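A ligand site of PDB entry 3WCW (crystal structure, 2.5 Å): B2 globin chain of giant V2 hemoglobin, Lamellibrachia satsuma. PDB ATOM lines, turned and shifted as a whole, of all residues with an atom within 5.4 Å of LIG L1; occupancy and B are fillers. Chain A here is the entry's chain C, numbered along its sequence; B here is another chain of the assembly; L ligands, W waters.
Merely in contact with LIG L1: Leu 50, Phe 51, Val 54, His 67, Arg 70, Val 71, Leu 75, Gln 98, Arg 102, Val 105, Gly 109, Phe 110, Ile 113, Thr 141 and Met 144. Hydrophobic or aromatic side chains within 4 Å of LIG L1: Leu 50, Phe 51, Val 54, His 67, Val 71, Leu 75, His 99, Val 105, Phe 110, Ile 113, Met 144 and His 90 of chain B. Of the 27 residues printed, 19 come within 4 Å of LIG L1.
The side-chain hydroxyl (OG1) of Thr 141 lies within hydrogen-bond range of the backbone carbonyl oxygen (O) of Phe 137, at 3.5 Å. O of Leu 95 sits at hydrogen-bond distance from ND1 of His 99 (2.8 Å). O of Gln 98 sits at hydrogen-bond distance from NE of Arg 102. A ring nitrogen (NE2) of His 90 of chain B lies within hydrogen-bond range of the side-chain amide nitrogen (NE2) of Gln 94 of chain B (3.5 Å).
An oxygen (O1) of LG2 L2 binds an iron atom (FE1) of LIG L1, 1.8 Å away.
Water W1 lies within hydrogen-bond range of the guanidinium group (NE) of Arg 70, a ring nitrogen (ND1) of His 67 and an oxygen (O4) of LIG L1.
NE2 of Gln 94 of chain B sits at hydrogen-bond distance from O1 of LIG L1. An oxygen (O2) of LG2 L2 is in hydrogen-bond range of a ring nitrogen (NE2) of His 67, at 2.9 Å. A ring nitrogen (NE2) of His 99 is bound to an iron atom (FE1) of LIG L1. The side-chain amide nitrogen (NE2) of Gln 98 sits at hydrogen-bond distance from an oxygen (O1) of LG3 L3, at 3.2 Å. NE of Arg 53 is in salt-bridge range of O3 of LIG L1 (2.7 Å). NE2 of His 90 of chain B lies within hydrogen-bond range of O1 of LIG L1 (2.9 Å).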
ATOM      1  N   LEU A  40      -6.384 -29.690  14.354  1.00  0.00           N
ATOM      2  CA  LEU A  40      -7.127 -30.722  13.634  1.00  0.00           C
ATOM      3  C   LEU A  40      -6.548 -30.907  12.233  1.00  0.00           C
ATOM      4  O   LEU A  40      -6.292 -32.030  11.778  1.00  0.00           O
ATOM      5  CB  LEU A  40      -8.618 -30.329  13.528  1.00  0.00           C
ATOM      6  CG  LEU A  40      -9.512 -31.301  12.746  1.00  0.00           C
ATOM      7  CD1 LEU A  40      -9.493 -32.658  13.411  1.00  0.00           C
ATOM      8  CD2 LEU A  40     -10.936 -30.763  12.666  1.00  0.00           C
ATOM      9  N   LEU A  50     -12.959 -29.454   3.950  1.00  0.00           N
ATOM     10  CA  LEU A  50     -14.378 -29.452   4.311  1.00  0.00           C
ATOM     11  C   LEU A  50     -14.828 -28.035   4.658  1.00  0.00           C
ATOM     12  O   LEU A  50     -16.018 -27.771   4.791  1.00  0.00           O
ATOM     13  CB  LEU A  50     -14.631 -30.359   5.510  1.00  0.00           C
ATOM     14  CG  LEU A  50     -14.167 -31.819   5.392  1.00  0.00           C
ATOM     15  CD1 LEU A  50     -14.173 -32.457   6.773  1.00  0.00           C
ATOM     16  CD2 LEU A  50     -15.077 -32.569   4.440  1.00  0.00           C
ATOM     17  N   PHE A  51     -13.854 -27.123   4.779  1.00  0.00           N
ATOM     18  CA  PHE A  51     -14.147 -25.745   5.155  1.00  0.00           C
ATOM     19  C   PHE A  51     -13.760 -24.746   4.069  1.00  0.00           C
ATOM     20  O   PHE A  51     -13.337 -23.607   4.339  1.00  0.00           O
ATOM     21  CB  PHE A  51     -13.415 -25.434   6.468  1.00  0.00           C
ATOM     22  CG  PHE A  51     -13.657 -26.476   7.538  1.00  0.00           C
ATOM     23  CD1 PHE A  51     -14.824 -26.456   8.298  1.00  0.00           C
ATOM     24  CD2 PHE A  51     -12.747 -27.524   7.724  1.00  0.00           C
ATOM     25  CE1 PHE A  51     -15.088 -27.469   9.215  1.00  0.00           C
ATOM     26  CE2 PHE A  51     -13.003 -28.539   8.635  1.00  0.00           C
ATOM     27  CZ  PHE A  51     -14.184 -28.514   9.394  1.00  0.00           C
ATOM     28  N   ARG A  53     -15.765 -23.291   2.025  1.00  0.00           N
ATOM     29  CA  ARG A  53     -16.743 -22.210   2.052  1.00  0.00           C
ATOM     30  C   ARG A  53     -16.413 -21.110   3.087  1.00  0.00           C
ATOM     31  O   ARG A  53     -16.821 -19.962   2.921  1.00  0.00           O
ATOM     32  CB  ARG A  53     -18.137 -22.789   2.328  1.00  0.00           C
ATOM     33  CG  ARG A  53     -19.275 -21.924   1.836  1.00  0.00           C
ATOM     34  CD  ARG A  53     -20.540 -22.301   2.533  1.00  0.00           C
ATOM     35  NE  ARG A  53     -20.479 -21.918   3.940  1.00  0.00           N
ATOM     36  CZ  ARG A  53     -20.637 -20.681   4.389  1.00  0.00           C
ATOM     37  NH1 ARG A  53     -20.545 -20.430   5.691  1.00  0.00           N
ATOM     38  NH2 ARG A  53     -20.910 -19.687   3.554  1.00  0.00           N
ATOM     39  N   VAL A  54     -15.688 -21.464   4.144  1.00  0.00           N
ATOM     40  CA  VAL A  54     -15.307 -20.511   5.184  1.00  0.00           C
ATOM     41  C   VAL A  54     -13.806 -20.192   5.139  1.00  0.00           C
ATOM     42  O   VAL A  54     -13.245 -19.653   6.089  1.00  0.00           O
ATOM     43  CB  VAL A  54     -15.655 -21.056   6.597  1.00  0.00           C
ATOM     44  CG1 VAL A  54     -17.168 -21.144   6.766  1.00  0.00           C
ATOM     45  CG2 VAL A  54     -15.022 -22.419   6.811  1.00  0.00           C
ATOM     46  N   HIS A  67     -16.481 -18.224  11.143  1.00  0.00           N
ATOM     47  CA  HIS A  67     -16.813 -19.630  11.316  1.00  0.00           C
ATOM     48  C   HIS A  67     -16.397 -20.138  12.707  1.00  0.00           C
ATOM     49  O   HIS A  67     -17.172 -20.815  13.388  1.00  0.00           O
ATOM     50  CB  HIS A  67     -16.124 -20.455  10.233  1.00  0.00           C
ATOM     51  CG  HIS A  67     -16.208 -21.927  10.475  1.00  0.00           C
ATOM     52  ND1 HIS A  67     -17.389 -22.626  10.408  1.00  0.00           N
ATOM     53  CD2 HIS A  67     -15.253 -22.821  10.820  1.00  0.00           C
ATOM     54  CE1 HIS A  67     -17.160 -23.898  10.711  1.00  0.00           C
ATOM     55  NE2 HIS A  67     -15.875 -24.042  10.957  1.00  0.00           N
ATOM     56  N   ARG A  70     -18.671 -19.058  15.282  1.00  0.00           N
ATOM     57  CA  ARG A  70     -19.902 -19.870  15.263  1.00  0.00           C
ATOM     58  C   ARG A  70     -19.654 -21.236  15.902  1.00  0.00           C
ATOM     59  O   ARG A  70     -20.526 -21.761  16.601  1.00  0.00           O
ATOM     60  CB  ARG A  70     -20.435 -20.064  13.822  1.00  0.00           C
ATOM     61  CG  ARG A  70     -20.984 -18.788  13.176  1.00  0.00           C
ATOM     62  CD  ARG A  70     -21.718 -19.066  11.863  1.00  0.00           C
ATOM     63  NE  ARG A  70     -20.846 -19.498  10.755  1.00  0.00           N
ATOM     64  CZ  ARG A  70     -20.114 -18.682   9.999  1.00  0.00           C
ATOM     65  NH1 ARG A  70     -20.137 -17.372  10.211  1.00  0.00           N
ATOM     66  NH2 ARG A  70     -19.350 -19.190   9.032  1.00  0.00           N
ATOM     67  N   VAL A  71     -18.491 -21.826  15.667  1.00  0.00           N
ATOM     68  CA  VAL A  71     -18.209 -23.117  16.269  1.00  0.00           C
ATOM     69  C   VAL A  71     -18.190 -22.982  17.787  1.00  0.00           C
ATOM     70  O   VAL A  71     -18.841 -23.740  18.506  1.00  0.00           O
ATOM     71  CB  VAL A  71     -16.862 -23.684  15.795  1.00  0.00           C
ATOM     72  CG1 VAL A  71     -16.564 -25.001  16.542  1.00  0.00           C
ATOM     73  CG2 VAL A  71     -16.911 -23.927  14.300  1.00  0.00           C
ATOM     74  N   GLY A  74     -21.555 -22.343  19.312  1.00  0.00           N
ATOM     75  CA  GLY A  74     -22.304 -23.586  19.366  1.00  0.00           C
ATOM     76  C   GLY A  74     -21.862 -24.492  20.504  1.00  0.00           C
ATOM     77  O   GLY A  74     -22.698 -25.173  21.112  1.00  0.00           O
ATOM     78  N   LEU A  75     -20.570 -24.511  20.774  1.00  0.00           N
ATOM     79  CA  LEU A  75     -20.044 -25.338  21.854  1.00  0.00           C
ATOM     80  C   LEU A  75     -20.409 -24.673  23.200  1.00  0.00           C
ATOM     81  O   LEU A  75     -20.679 -25.357  24.193  1.00  0.00           O
ATOM     82  CB  LEU A  75     -18.515 -25.472  21.727  1.00  0.00           C
ATOM     83  CG  LEU A  75     -17.955 -26.357  22.838  1.00  0.00           C
ATOM     84  CD1 LEU A  75     -18.605 -27.724  22.768  1.00  0.00           C
ATOM     85  CD2 LEU A  75     -16.441 -26.465  22.731  1.00  0.00           C
ATOM     86  N   LEU A  95     -27.877 -29.277  15.553  1.00  0.00           N
ATOM     87  CA  LEU A  95     -26.470 -29.220  15.170  1.00  0.00           C
ATOM     88  C   LEU A  95     -26.161 -30.409  14.286  1.00  0.00           C
ATOM     89  O   LEU A  95     -25.338 -30.344  13.379  1.00  0.00           O
ATOM     90  CB  LEU A  95     -25.556 -29.217  16.402  1.00  0.00           C
ATOM     91  CG  LEU A  95     -25.495 -27.892  17.183  1.00  0.00           C
ATOM     92  CD1 LEU A  95     -24.769 -28.115  18.500  1.00  0.00           C
ATOM     93  CD2 LEU A  95     -24.781 -26.850  16.349  1.00  0.00           C
ATOM     94  N   GLN A  98     -27.127 -29.939  10.820  1.00  0.00           N
ATOM     95  CA  GLN A  98     -26.239 -28.936  10.231  1.00  0.00           C
ATOM     96  C   GLN A  98     -24.943 -29.601   9.748  1.00  0.00           C
ATOM     97  O   GLN A  98     -24.312 -29.110   8.816  1.00  0.00           O
ATOM     98  CB  GLN A  98     -25.890 -27.840  11.225  1.00  0.00           C
ATOM     99  CG  GLN A  98     -27.025 -26.871  11.542  1.00  0.00           C
ATOM    100  CD  GLN A  98     -26.560 -25.665  12.326  1.00  0.00           C
ATOM    101  OE1 GLN A  98     -25.807 -25.798  13.285  1.00  0.00           O
ATOM    102  NE2 GLN A  98     -27.015 -24.495  11.934  1.00  0.00           N
ATOM    103  N   HIS A  99     -24.571 -30.703  10.388  1.00  0.00           N
ATOM    104  CA  HIS A  99     -23.347 -31.402  10.009  1.00  0.00           C
ATOM    105  C   HIS A  99     -23.602 -32.569   9.076  1.00  0.00           C
ATOM    106  O   HIS A  99     -22.667 -33.205   8.580  1.00  0.00           O
ATOM    107  CB  HIS A  99     -22.602 -31.873  11.268  1.00  0.00           C
ATOM    108  CG  HIS A  99     -21.958 -30.765  12.032  1.00  0.00           C
ATOM    109  ND1 HIS A  99     -22.680 -29.862  12.783  1.00  0.00           N
ATOM    110  CD2 HIS A  99     -20.670 -30.363  12.102  1.00  0.00           C
ATOM    111  CE1 HIS A  99     -21.869 -28.947  13.274  1.00  0.00           C
ATOM    112  NE2 HIS A  99     -20.636 -29.231  12.876  1.00  0.00           N
ATOM    113  N   ARG A 102     -23.184 -33.270   4.375  1.00  0.00           N
ATOM    114  CA  ARG A 102     -21.889 -32.666   4.114  1.00  0.00           C
ATOM    115  C   ARG A 102     -20.952 -33.853   4.144  1.00  0.00           C
ATOM    116  O   ARG A 102     -20.498 -34.277   5.206  1.00  0.00           O
ATOM    117  CB  ARG A 102     -21.510 -31.675   5.218  1.00  0.00           C
ATOM    118  CG  ARG A 102     -22.361 -30.430   5.272  1.00  0.00           C
ATOM    119  CD  ARG A 102     -21.885 -29.519   6.395  1.00  0.00           C
ATOM    120  NE  ARG A 102     -22.814 -28.421   6.671  1.00  0.00           N
ATOM    121  CZ  ARG A 102     -23.001 -27.366   5.885  1.00  0.00           C
ATOM    122  NH1 ARG A 102     -23.871 -26.424   6.245  1.00  0.00           N
ATOM    123  NH2 ARG A 102     -22.327 -27.251   4.745  1.00  0.00           N
ATOM    124  N   GLY A 104     -17.874 -36.357   4.083  1.00  0.00           N
ATOM    125  CA  GLY A 104     -16.602 -36.192   4.747  1.00  0.00           C
ATOM    126  C   GLY A 104     -16.749 -36.026   6.243  1.00  0.00           C
ATOM    127  O   GLY A 104     -16.062 -36.677   7.012  1.00  0.00           O
ATOM    128  N   VAL A 105     -17.664 -35.145   6.653  1.00  0.00           N
ATOM    129  CA  VAL A 105     -17.934 -34.906   8.069  1.00  0.00           C
ATOM    130  C   VAL A 105     -18.455 -36.197   8.682  1.00  0.00           C
ATOM    131  O   VAL A 105     -19.616 -36.552   8.473  1.00  0.00           O
ATOM    132  CB  VAL A 105     -19.003 -33.825   8.261  1.00  0.00           C
ATOM    133  CG1 VAL A 105     -19.289 -33.626   9.739  1.00  0.00           C
ATOM    134  CG2 VAL A 105     -18.556 -32.524   7.602  1.00  0.00           C
ATOM    135  N   THR A 106     -17.607 -36.887   9.451  1.00  0.00           N
ATOM    136  CA  THR A 106     -17.997 -38.153  10.068  1.00  0.00           C
ATOM    137  C   THR A 106     -17.633 -38.251  11.545  1.00  0.00           C
ATOM    138  O   THR A 106     -17.045 -37.333  12.120  1.00  0.00           O
ATOM    139  CB  THR A 106     -17.306 -39.325   9.351  1.00  0.00           C
ATOM    140  OG1 THR A 106     -15.897 -39.293   9.632  1.00  0.00           O
ATOM    141  CG2 THR A 106     -17.508 -39.211   7.855  1.00  0.00           C
ATOM    142  N   GLY A 109     -13.993 -37.469  12.295  1.00  0.00           N
ATOM    143  CA  GLY A 109     -13.530 -36.114  12.482  1.00  0.00           C
ATOM    144  C   GLY A 109     -13.756 -35.602  13.894  1.00  0.00           C
ATOM    145  O   GLY A 109     -12.912 -34.897  14.458  1.00  0.00           O
ATOM    146  N   PHE A 110     -14.905 -35.952  14.480  1.00  0.00           N
ATOM    147  CA  PHE A 110     -15.227 -35.516  15.820  1.00  0.00           C
ATOM    148  C   PHE A 110     -14.283 -36.152  16.832  1.00  0.00           C
ATOM    149  O   PHE A 110     -13.916 -35.511  17.814  1.00  0.00           O
ATOM    150  CB  PHE A 110     -16.681 -35.852  16.157  1.00  0.00           C
ATOM    151  CG  PHE A 110     -17.674 -34.884  15.558  1.00  0.00           C
ATOM    152  CD1 PHE A 110     -18.196 -33.854  16.325  1.00  0.00           C
ATOM    153  CD2 PHE A 110     -18.041 -34.987  14.221  1.00  0.00           C
ATOM    154  CE1 PHE A 110     -19.081 -32.929  15.761  1.00  0.00           C
ATOM    155  CE2 PHE A 110     -18.927 -34.071  13.643  1.00  0.00           C
ATOM    156  CZ  PHE A 110     -19.449 -33.041  14.409  1.00  0.00           C
ATOM    157  N   ILE A 113     -11.251 -33.999  16.501  1.00  0.00           N
ATOM    158  CA  ILE A 113     -11.348 -32.689  17.110  1.00  0.00           C
ATOM    159  C   ILE A 113     -11.346 -32.816  18.643  1.00  0.00           C
ATOM    160  O   ILE A 113     -10.847 -31.927  19.347  1.00  0.00           O
ATOM    161  CB  ILE A 113     -12.593 -31.911  16.601  1.00  0.00           C
ATOM    162  CG1 ILE A 113     -12.324 -30.414  16.707  1.00  0.00           C
ATOM    163  CG2 ILE A 113     -13.848 -32.309  17.385  1.00  0.00           C
ATOM    164  CD1 ILE A 113     -13.321 -29.564  15.970  1.00  0.00           C
ATOM    165  N   PHE A 117      -9.072 -30.580  21.078  1.00  0.00           N
ATOM    166  CA  PHE A 117      -9.498 -29.816  22.246  1.00  0.00           C
ATOM    167  C   PHE A 117      -8.718 -30.266  23.474  1.00  0.00           C
ATOM    168  O   PHE A 117      -8.344 -29.458  24.317  1.00  0.00           O
ATOM    169  CB  PHE A 117     -11.000 -29.977  22.472  1.00  0.00           C
ATOM    170  CG  PHE A 117     -11.818 -28.871  21.871  1.00  0.00           C
ATOM    171  CD1 PHE A 117     -11.899 -27.632  22.495  1.00  0.00           C
ATOM    172  CD2 PHE A 117     -12.477 -29.055  20.664  1.00  0.00           C
ATOM    173  CE1 PHE A 117     -12.631 -26.592  21.926  1.00  0.00           C
ATOM    174  CE2 PHE A 117     -13.222 -28.032  20.086  1.00  0.00           C
ATOM    175  CZ  PHE A 117     -13.298 -26.795  20.717  1.00  0.00           C
ATOM    176  N   PHE A 137     -17.640 -33.865  26.745  1.00  0.00           N
ATOM    177  CA  PHE A 137     -17.410 -33.439  25.364  1.00  0.00           C
ATOM    178  C   PHE A 137     -18.031 -34.527  24.489  1.00  0.00           C
ATOM    179  O   PHE A 137     -18.799 -34.232  23.581  1.00  0.00           O
ATOM    180  CB  PHE A 137     -15.904 -33.338  25.052  1.00  0.00           C
ATOM    181  CG  PHE A 137     -15.601 -32.656  23.741  1.00  0.00           C
ATOM    182  CD1 PHE A 137     -15.509 -31.263  23.671  1.00  0.00           C
ATOM    183  CD2 PHE A 137     -15.447 -33.393  22.572  1.00  0.00           C
ATOM    184  CE1 PHE A 137     -15.270 -30.617  22.458  1.00  0.00           C
ATOM    185  CE2 PHE A 137     -15.201 -32.749  21.354  1.00  0.00           C
ATOM    186  CZ  PHE A 137     -15.120 -31.363  21.288  1.00  0.00           C
ATOM    187  N   ILE A 140     -21.637 -34.587  24.412  1.00  0.00           N
ATOM    188  CA  ILE A 140     -22.037 -33.540  23.482  1.00  0.00           C
ATOM    189  C   ILE A 140     -21.899 -33.983  22.016  1.00  0.00           C
ATOM    190  O   ILE A 140     -22.846 -33.833  21.238  1.00  0.00           O
ATOM    191  CB  ILE A 140     -21.209 -32.238  23.697  1.00  0.00           C
ATOM    192  CG1 ILE A 140     -21.596 -31.596  25.025  1.00  0.00           C
ATOM    193  CG2 ILE A 140     -21.433 -31.272  22.526  1.00  0.00           C
ATOM    194  CD1 ILE A 140     -20.909 -30.288  25.292  1.00  0.00           C
ATOM    195  N   THR A 141     -20.748 -34.527  21.651  1.00  0.00           N
ATOM    196  CA  THR A 141     -20.554 -34.954  20.264  1.00  0.00           C
ATOM    197  C   THR A 141     -21.519 -36.051  19.834  1.00  0.00           C
ATOM    198  O   THR A 141     -22.035 -36.028  18.721  1.00  0.00           O
ATOM    199  CB  THR A 141     -19.098 -35.402  19.958  1.00  0.00           C
ATOM    200  OG1 THR A 141     -18.694 -36.428  20.867  1.00  0.00           O
ATOM    201  CG2 THR A 141     -18.127 -34.209  20.047  1.00  0.00           C
ATOM    202  N   MET A 144     -24.388 -34.916  18.273  1.00  0.00           N
ATOM    203  CA  MET A 144     -24.106 -34.229  17.017  1.00  0.00           C
ATOM    204  C   MET A 144     -23.770 -35.197  15.883  1.00  0.00           C
ATOM    205  O   MET A 144     -23.966 -34.873  14.720  1.00  0.00           O
ATOM    206  CB  MET A 144     -22.952 -33.249  17.186  1.00  0.00           C
ATOM    207  CG  MET A 144     -23.207 -32.120  18.176  1.00  0.00           C
ATOM    208  SD  MET A 144     -21.698 -31.127  18.401  1.00  0.00           S
ATOM    209  CE  MET A 144     -21.738 -30.144  16.927  1.00  0.00           C
ATOM    210  N   HIS B  90     -24.015 -13.888   7.494  1.00  0.00           N
ATOM    211  CA  HIS B  90     -24.422 -15.279   7.700  1.00  0.00           C
ATOM    212  C   HIS B  90     -25.865 -15.268   8.208  1.00  0.00           C
ATOM    213  O   HIS B  90     -26.748 -15.882   7.626  1.00  0.00           O
ATOM    214  CB  HIS B  90     -23.515 -15.945   8.727  1.00  0.00           C
ATOM    215  CG  HIS B  90     -23.649 -17.438   8.769  1.00  0.00           C
ATOM    216  ND1 HIS B  90     -22.917 -18.276   7.956  1.00  0.00           N
ATOM    217  CD2 HIS B  90     -24.392 -18.252   9.560  1.00  0.00           C
ATOM    218  CE1 HIS B  90     -23.197 -19.529   8.246  1.00  0.00           C
ATOM    219  NE2 HIS B  90     -24.101 -19.546   9.214  1.00  0.00           N
ATOM    220  N   GLN B  94     -29.490 -17.010   6.872  1.00  0.00           N
ATOM    221  CA  GLN B  94     -30.368 -17.859   7.658  1.00  0.00           C
ATOM    222  C   GLN B  94     -31.800 -17.338   7.705  1.00  0.00           C
ATOM    223  O   GLN B  94     -32.715 -18.079   8.044  1.00  0.00           O
ATOM    224  CB  GLN B  94     -29.764 -18.052   9.058  1.00  0.00           C
ATOM    225  CG  GLN B  94     -28.337 -18.624   9.010  1.00  0.00           C
ATOM    226  CD  GLN B  94     -27.630 -18.724  10.369  1.00  0.00           C
ATOM    227  OE1 GLN B  94     -27.469 -17.720  11.072  1.00  0.00           O
ATOM    228  NE2 GLN B  94     -27.223 -19.928  10.733  1.00  0.00           N
HETATM  229  C1  LIG L   1     -20.472 -25.832  10.778  1.00  0.00           C
HETATM  230  C2  LIG L   1     -20.260 -26.318  15.475  1.00  0.00           C
HETATM  231  C3  LIG L   1     -17.291 -30.089  14.992  1.00  0.00           C
HETATM  232  C4  LIG L   1     -17.583 -29.591  10.242  1.00  0.00           C
HETATM  233  C5  LIG L   1     -20.692 -25.616  12.101  1.00  0.00           C
HETATM  234  C6  LIG L   1     -21.490 -24.581  12.594  1.00  0.00           C
HETATM  235  C7  LIG L   1     -21.456 -24.708  13.938  1.00  0.00           C
HETATM  236  C8  LIG L   1     -20.597 -25.854  14.280  1.00  0.00           C
HETATM  237  C9  LIG L   1     -22.163 -23.821  14.991  1.00  0.00           C
HETATM  238  C10 LIG L   1     -22.246 -23.527  11.779  1.00  0.00           C
HETATM  239  C11 LIG L   1     -23.633 -23.935  11.396  1.00  0.00           C
HETATM  240  C12 LIG L   1     -24.387 -22.880  10.567  1.00  0.00           C
HETATM  241  O1  LIG L   1     -24.580 -21.727  11.038  1.00  0.00           O
HETATM  242  O2  LIG L   1     -24.748 -23.205   9.470  1.00  0.00           O
HETATM  243  C13 LIG L   1     -19.415 -27.405  15.809  1.00  0.00           C
HETATM  244  C14 LIG L   1     -19.103 -27.818  17.166  1.00  0.00           C
HETATM  245  C15 LIG L   1     -18.214 -28.941  16.998  1.00  0.00           C
HETATM  246  C16 LIG L   1     -18.072 -29.112  15.594  1.00  0.00           C
HETATM  247  C17 LIG L   1     -19.608 -27.191  18.420  1.00  0.00           C
HETATM  248  C18 LIG L   1     -17.625 -29.675  18.102  1.00  0.00           C
HETATM  249  C19 LIG L   1     -18.265 -30.586  18.812  1.00  0.00           C
HETATM  250  C20 LIG L   1     -17.127 -30.283  13.641  1.00  0.00           C
HETATM  251  C21 LIG L   1     -16.276 -31.355  13.098  1.00  0.00           C
HETATM  252  C22 LIG L   1     -16.328 -31.239  11.686  1.00  0.00           C
HETATM  253  C23 LIG L   1     -17.258 -30.054  11.471  1.00  0.00           C
HETATM  254  C24 LIG L   1     -15.491 -32.368  13.931  1.00  0.00           C
HETATM  255  C25 LIG L   1     -15.690 -32.011  10.733  1.00  0.00           C
HETATM  256  C26 LIG L   1     -14.863 -33.019  10.623  1.00  0.00           C
HETATM  257  C27 LIG L   1     -18.398 -28.508   9.962  1.00  0.00           C
HETATM  258  C28 LIG L   1     -18.706 -28.020   8.564  1.00  0.00           C
HETATM  259  C29 LIG L   1     -19.528 -26.946   8.769  1.00  0.00           C
HETATM  260  C30 LIG L   1     -19.712 -26.794  10.210  1.00  0.00           C
HETATM  261  C31 LIG L   1     -18.174 -28.644   7.278  1.00  0.00           C
HETATM  262  C32 LIG L   1     -20.138 -26.027   7.730  1.00  0.00           C
HETATM  263  C33 LIG L   1     -19.254 -24.818   7.594  1.00  0.00           C
HETATM  264  C34 LIG L   1     -19.749 -23.821   6.664  1.00  0.00           C
HETATM  265  O3  LIG L   1     -19.616 -23.999   5.416  1.00  0.00           O
HETATM  266  O4  LIG L   1     -20.307 -22.809   7.119  1.00  0.00           O
HETATM  267  N1  LIG L   1     -20.137 -26.406  13.121  1.00  0.00           N
HETATM  268  N2  LIG L   1     -18.819 -28.142  14.872  1.00  0.00           N
HETATM  269  N3  LIG L   1     -17.698 -29.530  12.633  1.00  0.00           N
HETATM  270  N4  LIG L   1     -19.023 -27.750  10.888  1.00  0.00           N
HETATM  271 FE1  LIG L   1     -18.934 -27.973  12.874  1.00  0.00          FE
HETATM  272  O1  LG2 L   2     -17.496 -26.872  12.856  1.00  0.00           O
HETATM  273  O2  LG2 L   2     -16.519 -26.548  12.168  1.00  0.00           O
HETATM  274  C1  LG3 L   3     -33.716 -18.523  12.982  1.00  0.00           C
HETATM  275  C2  LG3 L   3     -30.928 -15.212  14.864  1.00  0.00           C
HETATM  276  C3  LG3 L   3     -34.426 -11.928  14.416  1.00  0.00           C
HETATM  277  C4  LG3 L   3     -37.255 -15.343  12.541  1.00  0.00           C
HETATM  278  C5  LG3 L   3     -32.642 -17.915  13.540  1.00  0.00           C
HETATM  279  C6  LG3 L   3     -31.440 -18.586  13.823  1.00  0.00           C
HETATM  280  C7  LG3 L   3     -30.639 -17.660  14.363  1.00  0.00           C
HETATM  281  C8  LG3 L   3     -31.351 -16.392  14.415  1.00  0.00           C
HETATM  282  C9  LG3 L   3     -29.188 -17.862  14.866  1.00  0.00           C
HETATM  283  C10 LG3 L   3     -31.121 -20.047  13.578  1.00  0.00           C
HETATM  284  C11 LG3 L   3     -30.653 -20.307  12.167  1.00  0.00           C
HETATM  285  C12 LG3 L   3     -30.340 -21.775  11.900  1.00  0.00           C
HETATM  286  O1  LG3 L   3     -29.350 -22.301  12.470  1.00  0.00           O
HETATM  287  O2  LG3 L   3     -31.078 -22.380  11.167  1.00  0.00           O
HETATM  288  C13 LG3 L   3     -31.620 -13.994  14.911  1.00  0.00           C
HETATM  289  C14 LG3 L   3     -31.044 -12.768  15.432  1.00  0.00           C
HETATM  290  C15 LG3 L   3     -32.092 -11.789  15.283  1.00  0.00           C
HETATM  291  C16 LG3 L   3     -33.188 -12.497  14.720  1.00  0.00           C
HETATM  292  C17 LG3 L   3     -29.675 -12.590  15.981  1.00  0.00           C
HETATM  293  C18 LG3 L   3     -31.941 -10.419  15.684  1.00  0.00           C
HETATM  294  C19 LG3 L   3     -32.505  -9.895  16.743  1.00  0.00           C
HETATM  295  C20 LG3 L   3     -35.507 -12.589  13.871  1.00  0.00           C
HETATM  296  C21 LG3 L   3     -36.788 -11.921  13.605  1.00  0.00           C
HETATM  297  C22 LG3 L   3     -37.650 -12.888  13.056  1.00  0.00           C
HETATM  298  C23 LG3 L   3     -36.805 -14.142  13.016  1.00  0.00           C
HETATM  299  C24 LG3 L   3     -37.105 -10.442  13.879  1.00  0.00           C
HETATM  300  C25 LG3 L   3     -38.939 -12.722  12.667  1.00  0.00           C
HETATM  301  C26 LG3 L   3     -40.086 -12.481  13.220  1.00  0.00           C
HETATM  302  C27 LG3 L   3     -36.530 -16.519  12.485  1.00  0.00           C
HETATM  303  C28 LG3 L   3     -37.069 -17.832  11.946  1.00  0.00           C
HETATM  304  C29 LG3 L   3     -36.040 -18.707  12.080  1.00  0.00           C
HETATM  305  C30 LG3 L   3     -34.915 -17.970  12.683  1.00  0.00           C
HETATM  306  C31 LG3 L   3     -38.457 -18.045  11.387  1.00  0.00           C
HETATM  307  C32 LG3 L   3     -36.020 -20.164  11.694  1.00  0.00           C
HETATM  308  C33 LG3 L   3     -36.243 -21.090  12.840  1.00  0.00           C
HETATM  309  C34 LG3 L   3     -36.196 -22.490  12.416  1.00  0.00           C
HETATM  310  O3  LG3 L   3     -35.096 -23.141  12.485  1.00  0.00           O
HETATM  311  O4  LG3 L   3     -37.236 -23.024  11.985  1.00  0.00           O
HETATM  312  N1  LG3 L   3     -32.616 -16.569  13.895  1.00  0.00           N
HETATM  313  N2  LG3 L   3     -32.884 -13.856  14.482  1.00  0.00           N
HETATM  314  N3  LG3 L   3     -35.564 -13.922  13.505  1.00  0.00           N
HETATM  315  N4  LG3 L   3     -35.251 -16.661  12.902  1.00  0.00           N
HETATM  316 FE1  LG3 L   3     -34.089 -15.245  13.693  1.00  0.00          FE
HETATM  317  O   HOH W   1     -19.921 -21.847   9.708  1.00  0.00           O
